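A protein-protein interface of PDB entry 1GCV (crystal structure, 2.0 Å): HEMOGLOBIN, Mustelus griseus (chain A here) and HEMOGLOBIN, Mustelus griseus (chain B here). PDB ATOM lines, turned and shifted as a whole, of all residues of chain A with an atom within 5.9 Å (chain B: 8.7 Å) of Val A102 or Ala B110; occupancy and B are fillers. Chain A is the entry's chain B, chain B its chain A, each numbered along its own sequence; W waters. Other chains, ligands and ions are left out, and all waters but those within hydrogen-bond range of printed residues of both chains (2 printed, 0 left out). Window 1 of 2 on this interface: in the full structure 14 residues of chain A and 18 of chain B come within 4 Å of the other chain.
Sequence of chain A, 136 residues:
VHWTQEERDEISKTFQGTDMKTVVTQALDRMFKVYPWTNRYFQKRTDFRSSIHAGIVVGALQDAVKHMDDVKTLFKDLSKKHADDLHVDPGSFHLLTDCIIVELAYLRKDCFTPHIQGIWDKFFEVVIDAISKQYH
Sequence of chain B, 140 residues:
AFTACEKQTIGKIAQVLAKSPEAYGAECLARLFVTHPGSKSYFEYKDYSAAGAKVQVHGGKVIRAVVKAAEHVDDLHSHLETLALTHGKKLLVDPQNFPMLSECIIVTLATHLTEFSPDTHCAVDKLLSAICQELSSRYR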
ATOM      1  N   ARG A  30     -23.846  34.522  -9.719  1.00  0.00           N
ATOM      2  CA  ARG A  30     -24.721  34.055 -10.787  1.00  0.00           C
ATOM      3  C   ARG A  30     -26.134  33.980 -10.228  1.00  0.00           C
ATOM      4  O   ARG A  30     -27.088  34.425 -10.859  1.00  0.00           O
ATOM      5  CB  ARG A  30     -24.281  32.667 -11.263  1.00  0.00           C
ATOM      6  CG  ARG A  30     -25.110  32.107 -12.404  1.00  0.00           C
ATOM      7  CD  ARG A  30     -24.499  30.823 -12.945  1.00  0.00           C
ATOM      8  NE  ARG A  30     -23.176  31.049 -13.516  1.00  0.00           N
ATOM      9  CZ  ARG A  30     -22.956  31.402 -14.778  1.00  0.00           C
ATOM     10  NH1 ARG A  30     -23.973  31.570 -15.610  1.00  0.00           N
ATOM     11  NH2 ARG A  30     -21.716  31.593 -15.205  1.00  0.00           N
ATOM     12  N   THR A  97     -27.028  25.642  -5.307  1.00  0.00           N
ATOM     13  CA  THR A  97     -26.380  24.415  -5.766  1.00  0.00           C
ATOM     14  C   THR A  97     -26.528  24.238  -7.281  1.00  0.00           C
ATOM     15  O   THR A  97     -25.624  23.723  -7.936  1.00  0.00           O
ATOM     16  CB  THR A  97     -26.909  23.155  -5.008  1.00  0.00           C
ATOM     17  OG1 THR A  97     -28.320  23.007  -5.203  1.00  0.00           O
ATOM     18  CG2 THR A  97     -26.630  23.284  -3.532  1.00  0.00           C
ATOM     19  N   ASP A  98     -27.654  24.676  -7.842  1.00  0.00           N
ATOM     20  CA  ASP A  98     -27.860  24.587  -9.286  1.00  0.00           C
ATOM     21  C   ASP A  98     -26.862  25.510  -9.984  1.00  0.00           C
ATOM     22  O   ASP A  98     -26.366  25.198 -11.064  1.00  0.00           O
ATOM     23  CB  ASP A  98     -29.272  25.039  -9.672  1.00  0.00           C
ATOM     24  CG  ASP A  98     -30.296  23.936  -9.545  1.00  0.00           C
ATOM     25  OD1 ASP A  98     -29.896  22.784  -9.282  1.00  0.00           O
ATOM     26  OD2 ASP A  98     -31.502  24.230  -9.705  1.00  0.00           O
ATOM     27  N   CYS A  99     -26.580  26.657  -9.373  1.00  0.00           N
ATOM     28  CA  CYS A  99     -25.639  27.600  -9.963  1.00  0.00           C
ATOM     29  C   CYS A  99     -24.214  27.084  -9.855  1.00  0.00           C
ATOM     30  O   CYS A  99     -23.386  27.370 -10.720  1.00  0.00           O
ATOM     31  CB  CYS A  99     -25.762  28.968  -9.301  1.00  0.00           C
ATOM     32  SG  CYS A  99     -27.123  29.926  -9.980  1.00  0.00           S
ATOM     33  N   ILE A 100     -23.936  26.326  -8.794  1.00  0.00           N
ATOM     34  CA  ILE A 100     -22.612  25.731  -8.602  1.00  0.00           C
ATOM     35  C   ILE A 100     -22.396  24.681  -9.700  1.00  0.00           C
ATOM     36  O   ILE A 100     -21.293  24.532 -10.223  1.00  0.00           O
ATOM     37  CB  ILE A 100     -22.478  25.050  -7.211  1.00  0.00           C
ATOM     38  CG1 ILE A 100     -22.456  26.114  -6.108  1.00  0.00           C
ATOM     39  CG2 ILE A 100     -21.195  24.212  -7.160  1.00  0.00           C
ATOM     40  CD1 ILE A 100     -22.481  25.553  -4.702  1.00  0.00           C
ATOM     41  N   ILE A 101     -23.455  23.959 -10.060  1.00  0.00           N
ATOM     42  CA  ILE A 101     -23.337  22.965 -11.113  1.00  0.00           C
ATOM     43  C   ILE A 101     -23.058  23.661 -12.451  1.00  0.00           C
ATOM     44  O   ILE A 101     -22.283  23.155 -13.268  1.00  0.00           O
ATOM     45  CB  ILE A 101     -24.610  22.084 -11.196  1.00  0.00           C
ATOM     46  CG1 ILE A 101     -24.477  20.914 -10.217  1.00  0.00           C
ATOM     47  CG2 ILE A 101     -24.808  21.542 -12.612  1.00  0.00           C
ATOM     48  CD1 ILE A 101     -25.787  20.316  -9.789  1.00  0.00           C
ATOM     49  N   VAL A 102     -23.665  24.826 -12.673  1.00  0.00           N
ATOM     50  CA  VAL A 102     -23.435  25.557 -13.918  1.00  0.00           C
ATOM     51  C   VAL A 102     -21.977  26.025 -13.983  1.00  0.00           C
ATOM     52  O   VAL A 102     -21.350  25.990 -15.045  1.00  0.00           O
ATOM     53  CB  VAL A 102     -24.362  26.784 -14.035  1.00  0.00           C
ATOM     54  CG1 VAL A 102     -23.854  27.724 -15.114  1.00  0.00           C
ATOM     55  CG2 VAL A 102     -25.777  26.333 -14.358  1.00  0.00           C
ATOM     56  N   GLU A 103     -21.446  26.470 -12.844  1.00  0.00           N
ATOM     57  CA  GLU A 103     -20.054  26.926 -12.769  1.00  0.00           C
ATOM     58  C   GLU A 103     -19.097  25.743 -12.931  1.00  0.00           C
ATOM     59  O   GLU A 103     -18.042  25.887 -13.539  1.00  0.00           O
ATOM     60  CB  GLU A 103     -19.767  27.629 -11.432  1.00  0.00           C
ATOM     61  CG  GLU A 103     -20.424  28.997 -11.260  1.00  0.00           C
ATOM     62  CD  GLU A 103     -20.028  29.978 -12.333  1.00  0.00           C
ATOM     63  OE1 GLU A 103     -20.799  30.923 -12.586  1.00  0.00           O
ATOM     64  OE2 GLU A 103     -18.944  29.806 -12.923  1.00  0.00           O
ATOM     65  N   LEU A 104     -19.447  24.582 -12.381  1.00  0.00           N
ATOM     66  CA  LEU A 104     -18.590  23.407 -12.530  1.00  0.00           C
ATOM     67  C   LEU A 104     -18.580  22.995 -14.002  1.00  0.00           C
ATOM     68  O   LEU A 104     -17.543  22.595 -14.535  1.00  0.00           O
ATOM     69  CB  LEU A 104     -19.099  22.243 -11.680  1.00  0.00           C
ATOM     70  CG  LEU A 104     -18.651  22.212 -10.217  1.00  0.00           C
ATOM     71  CD1 LEU A 104     -19.266  21.008  -9.548  1.00  0.00           C
ATOM     72  CD2 LEU A 104     -17.125  22.149 -10.120  1.00  0.00           C
ATOM     73  N   ALA A 105     -19.742  23.102 -14.650  1.00  0.00           N
ATOM     74  CA  ALA A 105     -19.895  22.760 -16.062  1.00  0.00           C
ATOM     75  C   ALA A 105     -19.086  23.719 -16.924  1.00  0.00           C
ATOM     76  O   ALA A 105     -18.408  23.315 -17.869  1.00  0.00           O
ATOM     77  CB  ALA A 105     -21.367  22.823 -16.463  1.00  0.00           C
ATOM     78  N   TYR A 106     -19.169  24.998 -16.586  1.00  0.00           N
ATOM     79  CA  TYR A 106     -18.449  26.025 -17.310  1.00  0.00           C
ATOM     80  C   TYR A 106     -16.938  25.886 -17.133  1.00  0.00           C
ATOM     81  O   TYR A 106     -16.160  26.223 -18.026  1.00  0.00           O
ATOM     82  CB  TYR A 106     -18.885  27.398 -16.826  1.00  0.00           C
ATOM     83  CG  TYR A 106     -18.312  28.506 -17.659  1.00  0.00           C
ATOM     84  CD1 TYR A 106     -18.672  28.649 -18.997  1.00  0.00           C
ATOM     85  CD2 TYR A 106     -17.406  29.409 -17.116  1.00  0.00           C
ATOM     86  CE1 TYR A 106     -18.149  29.663 -19.771  1.00  0.00           C
ATOM     87  CE2 TYR A 106     -16.874  30.427 -17.880  1.00  0.00           C
ATOM     88  CZ  TYR A 106     -17.251  30.550 -19.207  1.00  0.00           C
ATOM     89  OH  TYR A 106     -16.731  31.572 -19.968  1.00  0.00           O
ATOM     90  N   LEU A 107     -16.531  25.388 -15.973  1.00  0.00           N
ATOM     91  CA  LEU A 107     -15.118  25.209 -15.670  1.00  0.00           C
ATOM     92  C   LEU A 107     -14.530  23.952 -16.309  1.00  0.00           C
ATOM     93  O   LEU A 107     -13.449  24.005 -16.891  1.00  0.00           O
ATOM     94  CB  LEU A 107     -14.903  25.161 -14.151  1.00  0.00           C
ATOM     95  CG  LEU A 107     -13.461  24.959 -13.681  1.00  0.00           C
ATOM     96  CD1 LEU A 107     -12.680  26.253 -13.862  1.00  0.00           C
ATOM     97  CD2 LEU A 107     -13.450  24.521 -12.226  1.00  0.00           C
ATOM     98  N   LYS A 109     -15.993  22.115 -18.780  1.00  0.00           N
ATOM     99  CA  LYS A 109     -16.416  21.978 -20.168  1.00  0.00           C
ATOM    100  C   LYS A 109     -16.798  20.548 -20.555  1.00  0.00           C
ATOM    101  O   LYS A 109     -17.537  19.881 -19.833  1.00  0.00           O
ATOM    102  CB  LYS A 109     -15.322  22.511 -21.092  1.00  0.00           C
ATOM    103  CG  LYS A 109     -15.566  23.942 -21.553  1.00  0.00           C
ATOM    104  CD  LYS A 109     -14.503  24.898 -21.038  1.00  0.00           C
ATOM    105  CE  LYS A 109     -15.042  26.321 -20.881  1.00  0.00           C
ATOM    106  NZ  LYS A 109     -16.470  26.461 -21.304  1.00  0.00           N
ATOM    107  N   TYR B  24     -25.993  19.094 -29.791  1.00  0.00           N
ATOM    108  CA  TYR B  24     -26.390  19.839 -28.599  1.00  0.00           C
ATOM    109  C   TYR B  24     -27.650  19.230 -27.970  1.00  0.00           C
ATOM    110  O   TYR B  24     -27.712  19.016 -26.754  1.00  0.00           O
ATOM    111  CB  TYR B  24     -26.677  21.302 -28.952  1.00  0.00           C
ATOM    112  CG  TYR B  24     -25.455  22.147 -29.223  1.00  0.00           C
ATOM    113  CD1 TYR B  24     -25.258  22.735 -30.470  1.00  0.00           C
ATOM    114  CD2 TYR B  24     -24.508  22.382 -28.230  1.00  0.00           C
ATOM    115  CE1 TYR B  24     -24.155  23.535 -30.722  1.00  0.00           C
ATOM    116  CE2 TYR B  24     -23.397  23.184 -28.474  1.00  0.00           C
ATOM    117  CZ  TYR B  24     -23.230  23.756 -29.720  1.00  0.00           C
ATOM    118  OH  TYR B  24     -22.144  24.559 -29.969  1.00  0.00           O
ATOM    119  N   GLU B  27     -27.065  15.929 -26.209  1.00  0.00           N
ATOM    120  CA  GLU B  27     -26.421  16.115 -24.922  1.00  0.00           C
ATOM    121  C   GLU B  27     -27.426  16.608 -23.877  1.00  0.00           C
ATOM    122  O   GLU B  27     -27.385  16.189 -22.723  1.00  0.00           O
ATOM    123  CB  GLU B  27     -25.258  17.104 -25.048  1.00  0.00           C
ATOM    124  CG  GLU B  27     -24.520  17.331 -23.738  1.00  0.00           C
ATOM    125  CD  GLU B  27     -23.308  18.223 -23.892  1.00  0.00           C
ATOM    126  OE1 GLU B  27     -22.742  18.270 -25.002  1.00  0.00           O
ATOM    127  OE2 GLU B  27     -22.923  18.874 -22.897  1.00  0.00           O
ATOM    128  N   ARG B  31     -28.438  14.496 -20.294  1.00  0.00           N
ATOM    129  CA  ARG B  31     -28.305  15.036 -18.951  1.00  0.00           C
ATOM    130  C   ARG B  31     -29.630  14.866 -18.232  1.00  0.00           C
ATOM    131  O   ARG B  31     -29.665  14.536 -17.047  1.00  0.00           O
ATOM    132  CB  ARG B  31     -27.921  16.512 -19.006  1.00  0.00           C
ATOM    133  CG  ARG B  31     -26.598  16.739 -19.681  1.00  0.00           C
ATOM    134  CD  ARG B  31     -26.030  18.104 -19.394  1.00  0.00           C
ATOM    135  NE  ARG B  31     -24.777  18.266 -20.120  1.00  0.00           N
ATOM    136  CZ  ARG B  31     -23.587  17.967 -19.618  1.00  0.00           C
ATOM    137  NH1 ARG B  31     -23.489  17.492 -18.384  1.00  0.00           N
ATOM    138  NH2 ARG B  31     -22.502  18.108 -20.364  1.00  0.00           N
ATOM    139  N   SER B 102     -35.193  22.349 -19.340  1.00  0.00           N
ATOM    140  CA  SER B 102     -34.643  23.694 -19.481  1.00  0.00           C
ATOM    141  C   SER B 102     -33.322  23.833 -18.720  1.00  0.00           C
ATOM    142  O   SER B 102     -32.385  24.452 -19.214  1.00  0.00           O
ATOM    143  CB  SER B 102     -35.645  24.739 -18.979  1.00  0.00           C
ATOM    144  OG  SER B 102     -36.721  24.859 -19.889  1.00  0.00           O
ATOM    145  N   GLU B 103     -33.244  23.258 -17.522  1.00  0.00           N
ATOM    146  CA  GLU B 103     -32.017  23.336 -16.738  1.00  0.00           C
ATOM    147  C   GLU B 103     -30.874  22.549 -17.382  1.00  0.00           C
ATOM    148  O   GLU B 103     -29.713  22.923 -17.248  1.00  0.00           O
ATOM    149  CB  GLU B 103     -32.250  22.834 -15.309  1.00  0.00           C
ATOM    150  CG  GLU B 103     -31.137  23.220 -14.326  1.00  0.00           C
ATOM    151  CD  GLU B 103     -30.813  24.722 -14.318  1.00  0.00           C
ATOM    152  OE1 GLU B 103     -29.624  25.074 -14.148  1.00  0.00           O
ATOM    153  OE2 GLU B 103     -31.740  25.548 -14.477  1.00  0.00           O
ATOM    154  N   CYS B 104     -31.201  21.467 -18.084  1.00  0.00           N
ATOM    155  CA  CYS B 104     -30.179  20.659 -18.746  1.00  0.00           C
ATOM    156  C   CYS B 104     -29.648  21.343 -20.001  1.00  0.00           C
ATOM    157  O   CYS B 104     -28.503  21.121 -20.394  1.00  0.00           O
ATOM    158  CB  CYS B 104     -30.734  19.281 -19.087  1.00  0.00           C
ATOM    159  SG  CYS B 104     -30.921  18.258 -17.629  1.00  0.00           S
ATOM    160  N   ILE B 105     -30.484  22.164 -20.634  1.00  0.00           N
ATOM    161  CA  ILE B 105     -30.071  22.923 -21.812  1.00  0.00           C
ATOM    162  C   ILE B 105     -29.093  23.981 -21.292  1.00  0.00           C
ATOM    163  O   ILE B 105     -28.069  24.260 -21.917  1.00  0.00           O
ATOM    164  CB  ILE B 105     -31.272  23.646 -22.501  1.00  0.00           C
ATOM    165  CG1 ILE B 105     -32.097  22.645 -23.312  1.00  0.00           C
ATOM    166  CG2 ILE B 105     -30.767  24.752 -23.428  1.00  0.00           C
ATOM    167  CD1 ILE B 105     -33.477  23.155 -23.692  1.00  0.00           C
ATOM    168  N   ILE B 106     -29.407  24.559 -20.134  1.00  0.00           N
ATOM    169  CA  ILE B 106     -28.540  25.573 -19.541  1.00  0.00           C
ATOM    170  C   ILE B 106     -27.173  24.958 -19.233  1.00  0.00           C
ATOM    171  O   ILE B 106     -26.146  25.541 -19.559  1.00  0.00           O
ATOM    172  CB  ILE B 106     -29.141  26.160 -18.228  1.00  0.00           C
ATOM    173  CG1 ILE B 106     -30.397  26.986 -18.530  1.00  0.00           C
ATOM    174  CG2 ILE B 106     -28.105  27.030 -17.518  1.00  0.00           C
ATOM    175  CD1 ILE B 106     -30.155  28.170 -19.435  1.00  0.00           C
ATOM    176  N   VAL B 107     -27.157  23.781 -18.613  1.00  0.00           N
ATOM    177  CA  VAL B 107     -25.894  23.129 -18.286  1.00  0.00           C
ATOM    178  C   VAL B 107     -25.131  22.776 -19.565  1.00  0.00           C
ATOM    179  O   VAL B 107     -23.902  22.907 -19.622  1.00  0.00           O
ATOM    180  CB  VAL B 107     -26.114  21.849 -17.444  1.00  0.00           C
ATOM    181  CG1 VAL B 107     -24.795  21.094 -17.276  1.00  0.00           C
ATOM    182  CG2 VAL B 107     -26.679  22.223 -16.075  1.00  0.00           C
ATOM    183  N   THR B 108     -25.855  22.345 -20.594  1.00  0.00           N
ATOM    184  CA  THR B 108     -25.220  21.998 -21.860  1.00  0.00           C
ATOM    185  C   THR B 108     -24.562  23.223 -22.488  1.00  0.00           C
ATOM    186  O   THR B 108     -23.462  23.126 -23.011  1.00  0.00           O
ATOM    187  CB  THR B 108     -26.235  21.406 -22.858  1.00  0.00           C
ATOM    188  OG1 THR B 108     -26.688  20.136 -22.371  1.00  0.00           O
ATOM    189  CG2 THR B 108     -25.601  21.225 -24.234  1.00  0.00           C
ATOM    190  N   LEU B 109     -25.228  24.372 -22.434  1.00  0.00           N
ATOM    191  CA  LEU B 109     -24.670  25.598 -23.004  1.00  0.00           C
ATOM    192  C   LEU B 109     -23.409  26.039 -22.254  1.00  0.00           C
ATOM    193  O   LEU B 109     -22.465  26.536 -22.862  1.00  0.00           O
ATOM    194  CB  LEU B 109     -25.707  26.733 -22.966  1.00  0.00           C
ATOM    195  CG  LEU B 109     -26.846  26.714 -23.990  1.00  0.00           C
ATOM    196  CD1 LEU B 109     -27.793  27.869 -23.719  1.00  0.00           C
ATOM    197  CD2 LEU B 109     -26.277  26.808 -25.385  1.00  0.00           C
ATOM    198  N   ALA B 110     -23.392  25.854 -20.935  1.00  0.00           N
ATOM    199  CA  ALA B 110     -22.241  26.235 -20.114  1.00  0.00           C
ATOM    200  C   ALA B 110     -20.982  25.439 -20.442  1.00  0.00           C
ATOM    201  O   ALA B 110     -19.881  25.973 -20.362  1.00  0.00           O
ATOM    202  CB  ALA B 110     -22.576  26.081 -18.636  1.00  0.00           C
ATOM    203  N   THR B 111     -21.137  24.169 -20.807  1.00  0.00           N
ATOM    204  CA  THR B 111     -19.983  23.326 -21.133  1.00  0.00           C
ATOM    205  C   THR B 111     -19.441  23.576 -22.537  1.00  0.00           C
ATOM    206  O   THR B 111     -18.342  23.132 -22.874  1.00  0.00           O
ATOM    207  CB  THR B 111     -20.312  21.811 -21.016  1.00  0.00           C
ATOM    208  OG1 THR B 111     -21.149  21.417 -22.107  1.00  0.00           O
ATOM    209  CG2 THR B 111     -21.015  21.507 -19.706  1.00  0.00           C
ATOM    210  N   HIS B 112     -20.212  24.292 -23.351  1.00  0.00           N
ATOM    211  CA  HIS B 112     -19.807  24.589 -24.720  1.00  0.00           C
ATOM    212  C   HIS B 112     -19.411  26.044 -24.916  1.00  0.00           C
ATOM    213  O   HIS B 112     -18.266  26.340 -25.252  1.00  0.00           O
ATOM    214  CB  HIS B 112     -20.932  24.223 -25.690  1.00  0.00           C
ATOM    215  CG  HIS B 112     -21.154  22.750 -25.815  1.00  0.00           C
ATOM    216  ND1 HIS B 112     -20.438  21.963 -26.691  1.00  0.00           N
ATOM    217  CD2 HIS B 112     -21.976  21.910 -25.141  1.00  0.00           C
ATOM    218  CE1 HIS B 112     -20.809  20.703 -26.552  1.00  0.00           C
ATOM    219  NE2 HIS B 112     -21.741  20.643 -25.616  1.00  0.00           N
ATOM    220  N   LEU B 113     -20.358  26.950 -24.700  1.00  0.00           N
ATOM    221  CA  LEU B 113     -20.112  28.379 -24.859  1.00  0.00           C
ATOM    222  C   LEU B 113     -18.820  28.861 -24.189  1.00  0.00           C
ATOM    223  O   LEU B 113     -18.485  28.449 -23.072  1.00  0.00           O
ATOM    224  CB  LEU B 113     -21.302  29.172 -24.316  1.00  0.00           C
ATOM    225  CG  LEU B 113     -22.409  29.524 -25.311  1.00  0.00           C
ATOM    226  CD1 LEU B 113     -22.577  28.425 -26.347  1.00  0.00           C
ATOM    227  CD2 LEU B 113     -23.699  29.736 -24.550  1.00  0.00           C
ATOM    228  N   THR B 114     -18.098  29.732 -24.894  1.00  0.00           N
ATOM    229  CA  THR B 114     -16.847  30.294 -24.396  1.00  0.00           C
ATOM    230  C   THR B 114     -17.179  31.220 -23.238  1.00  0.00           C
ATOM    231  O   THR B 114     -16.497  31.221 -22.219  1.00  0.00           O
ATOM    232  CB  THR B 114     -16.110  31.109 -25.493  1.00  0.00           C
ATOM    233  OG1 THR B 114     -17.066  31.763 -26.339  1.00  0.00           O
ATOM    234  CG2 THR B 114     -15.237  30.194 -26.341  1.00  0.00           C
ATOM    235  N   GLU B 115     -18.237  32.007 -23.404  1.00  0.00           N
ATOM    236  CA  GLU B 115     -18.667  32.922 -22.360  1.00  0.00           C
ATOM    237  C   GLU B 115     -20.114  32.633 -21.961  1.00  0.00           C
ATOM    238  O   GLU B 115     -21.012  32.599 -22.804  1.00  0.00           O
ATOM    239  CB  GLU B 115     -18.511  34.380 -22.827  1.00  0.00           C
ATOM    240  CG  GLU B 115     -19.760  35.014 -23.443  1.00  0.00           C
ATOM    241  CD  GLU B 115     -20.496  35.935 -22.476  1.00  0.00           C
ATOM    242  OE1 GLU B 115     -21.694  35.691 -22.205  1.00  0.00           O
ATOM    243  OE2 GLU B 115     -19.877  36.906 -21.986  1.00  0.00           O
ATOM    244  N   PHE B 116     -20.323  32.392 -20.670  1.00  0.00           N
ATOM    245  CA  PHE B 116     -21.656  32.127 -20.143  1.00  0.00           C
ATOM    246  C   PHE B 116     -21.804  32.846 -18.812  1.00  0.00           C
ATOM    247  O   PHE B 116     -21.887  32.229 -17.750  1.00  0.00           O
ATOM    248  CB  PHE B 116     -21.890  30.624 -19.961  1.00  0.00           C
ATOM    249  CG  PHE B 116     -23.347  30.245 -19.911  1.00  0.00           C
ATOM    250  CD1 PHE B 116     -24.192  30.528 -20.988  1.00  0.00           C
ATOM    251  CD2 PHE B 116     -23.885  29.637 -18.779  1.00  0.00           C
ATOM    252  CE1 PHE B 116     -25.550  30.216 -20.940  1.00  0.00           C
ATOM    253  CE2 PHE B 116     -25.246  29.320 -18.721  1.00  0.00           C
ATOM    254  CZ  PHE B 116     -26.078  29.612 -19.805  1.00  0.00           C
ATOM    255  N   SER B 117     -21.829  34.171 -18.890  1.00  0.00           N
ATOM    256  CA  SER B 117     -21.951  35.018 -17.717  1.00  0.00           C
ATOM    257  C   SER B 117     -23.384  35.037 -17.210  1.00  0.00           C
ATOM    258  O   SER B 117     -24.317  34.694 -17.941  1.00  0.00           O
ATOM    259  CB  SER B 117     -21.543  36.442 -18.069  1.00  0.00           C
ATOM    260  OG  SER B 117     -22.490  37.005 -18.962  1.00  0.00           O
ATOM    261  N   PRO B 118     -23.575  35.434 -15.944  1.00  0.00           N
ATOM    262  CA  PRO B 118     -24.905  35.507 -15.335  1.00  0.00           C
ATOM    263  C   PRO B 118     -25.946  36.216 -16.215  1.00  0.00           C
ATOM    264  O   PRO B 118     -27.116  35.839 -16.229  1.00  0.00           O
ATOM    265  CB  PRO B 118     -24.646  36.247 -14.030  1.00  0.00           C
ATOM    266  CG  PRO B 118     -23.260  35.853 -13.677  1.00  0.00           C
ATOM    267  CD  PRO B 118     -22.520  35.796 -14.982  1.00  0.00           C
ATOM    268  N   THR B 120     -26.041  36.398 -19.624  1.00  0.00           N
ATOM    269  CA  THR B 120     -26.395  35.553 -20.760  1.00  0.00           C
ATOM    270  C   THR B 120     -27.311  34.439 -20.254  1.00  0.00           C
ATOM    271  O   THR B 120     -28.306  34.090 -20.890  1.00  0.00           O
ATOM    272  CB  THR B 120     -25.120  34.948 -21.396  1.00  0.00           C
ATOM    273  OG1 THR B 120     -24.340  36.000 -21.976  1.00  0.00           O
ATOM    274  CG2 THR B 120     -25.471  33.932 -22.470  1.00  0.00           C
ATOM    275  N   HIS B 121     -26.949  33.903 -19.092  1.00  0.00           N
ATOM    276  CA  HIS B 121     -27.685  32.845 -18.406  1.00  0.00           C
ATOM    277  C   HIS B 121     -29.115  33.322 -18.164  1.00  0.00           C
ATOM    278  O   HIS B 121     -30.084  32.636 -18.475  1.00  0.00           O
ATOM    279  CB  HIS B 121     -26.989  32.556 -17.066  1.00  0.00           C
ATOM    280  CG  HIS B 121     -27.572  31.414 -16.288  1.00  0.00           C
ATOM    281  ND1 HIS B 121     -26.855  30.733 -15.329  1.00  0.00           N
ATOM    282  CD2 HIS B 121     -28.809  30.862 -16.294  1.00  0.00           C
ATOM    283  CE1 HIS B 121     -27.624  29.812 -14.777  1.00  0.00           C
ATOM    284  NE2 HIS B 121     -28.816  29.869 -15.344  1.00  0.00           N
ATOM    285  N   VAL B 124     -31.103  33.622 -21.432  1.00  0.00           N
ATOM    286  CA  VAL B 124     -31.442  32.300 -21.937  1.00  0.00           C
ATOM    287  C   VAL B 124     -32.500  31.630 -21.059  1.00  0.00           C
ATOM    288  O   VAL B 124     -33.434  30.997 -21.570  1.00  0.00           O
ATOM    289  CB  VAL B 124     -30.187  31.399 -22.008  1.00  0.00           C
ATOM    290  CG1 VAL B 124     -30.538  30.045 -22.604  1.00  0.00           C
ATOM    291  CG2 VAL B 124     -29.124  32.079 -22.844  1.00  0.00           C
ATOM    292  N   ASP B 125     -32.359  31.770 -19.742  1.00  0.00           N
ATOM    293  CA  ASP B 125     -33.312  31.175 -18.808  1.00  0.00           C
ATOM    294  C   ASP B 125     -34.699  31.773 -19.005  1.00  0.00           C
ATOM    295  O   ASP B 125     -35.703  31.086 -18.844  1.00  0.00           O
ATOM    296  CB  ASP B 125     -32.867  31.394 -17.356  1.00  0.00           C
ATOM    297  CG  ASP B 125     -33.503  30.399 -16.398  1.00  0.00           C
ATOM    298  OD1 ASP B 125     -33.512  29.191 -16.719  1.00  0.00           O
ATOM    299  OD2 ASP B 125     -33.995  30.820 -15.328  1.00  0.00           O
HETATM  300  O   HOH W   1     -27.878  23.612 -13.056  1.00  0.00           O
HETATM  301  O   HOH W   2     -18.530  33.493 -18.831  1.00  0.00           O
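Of the printed residues of chain B, Val A102 touches Ile B106, Ala B110 and His B121.
Of chain A, only Val A102 (3.8 Å), Ala A105 (3.9 Å), Tyr A106 (3.2 Å) and Lys A109 (3.6 Å) come within 4 Å of Ala B110.
Of the printed residues of chain A, Ser B117 touches Arg A30.
Of the printed residues of chain B, Tyr A106 touches Ala B110, Leu B113, Thr B114, Glu B115 and Phe B116.
Of the printed residues of chain A, Thr B114 touches Tyr A106 (2.3 Å).
Printed residues of chain A within 4 Å of Glu B115: Tyr A106 (3.4 Å).
The nearest printed residue of chain B that does not touch Val A102 is Glu B103 (4.1 Å).
The nearest residue of chain A that does not touch Ala B110 is Leu A107 (5.6 Å).
The nearest printed residue of chain A that does not touch Val B107 is Val A102 (4.5 Å).
Of the 13 printed residues of chain A, 6 touch a printed residue of chain B.
Printed residues of chain A that touch a printed residue of chain B: Arg A30, Ile A101, Val A102, Ala A105, Tyr A106 and Lys A109.
Among the printed residues, 19 pairs touch across the chains.
The backbone carbonyl oxygen (O) of Leu B113 lies within hydrogen-bond range of the side-chain amino group (NZ) of Lys A109 (3.3 Å).
The backbone carbonyl oxygen (O) of Phe B116 lies within hydrogen-bond range of the guanidinium group (NH2) of Arg A30.
ND1 of His B121 lies within hydrogen-bond range of NH1 of Arg A30.
OH of Tyr A106 sits close to O of Thr B114.
The side-chain hydroxyl (OG1) of Thr B111 sits at hydrogen-bond distance from the side-chain carboxylate (OE2) of Glu B27.
O of Thr B108 lies within hydrogen-bond range of OG1 of Thr B111 (3.0 Å).
The side-chain hydroxyl (OG1) of Thr B120 lies within hydrogen-bond range of the side-chain carboxylate (OE1) of Glu B115.
The guanidinium group (NE) of Arg A30 is in salt-bridge range of the side-chain carboxylate (OE1) of Glu A103 (2.6 Å).
O of Tyr A106 sits close to NZ of Lys A109, 3.3 Å away.
Water W1 bridges OE1 of Glu B103 (2.5 Å) and O of Asp A98 (3.0 Å).
Water W2 lies within hydrogen-bond range of the backbone NH (N) of Phe B116, the side-chain hydroxyl (OH) of Tyr A106 and the backbone NH (N) of Ser B117.
C of Ser B117 touches NH1 of Arg A30, 3.9 Å away.
Pro B118 touches Arg A30 (CG to CA, 3.7 Å).
Val B107 touches Ile A101.
Ile B106 touches Val A102.
Ala B110 touches Val A102.
Ala A105 touches Ala B110 (O to O, 3.9 Å).
CB of Ala A105 touches CG2 of Thr B111 (3.5 Å).
Tyr A106 touches Ala B110.
Leu B113 touches Tyr A106.
Ala B110 touches Lys A109 (O to NZ, 3.6 Å).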
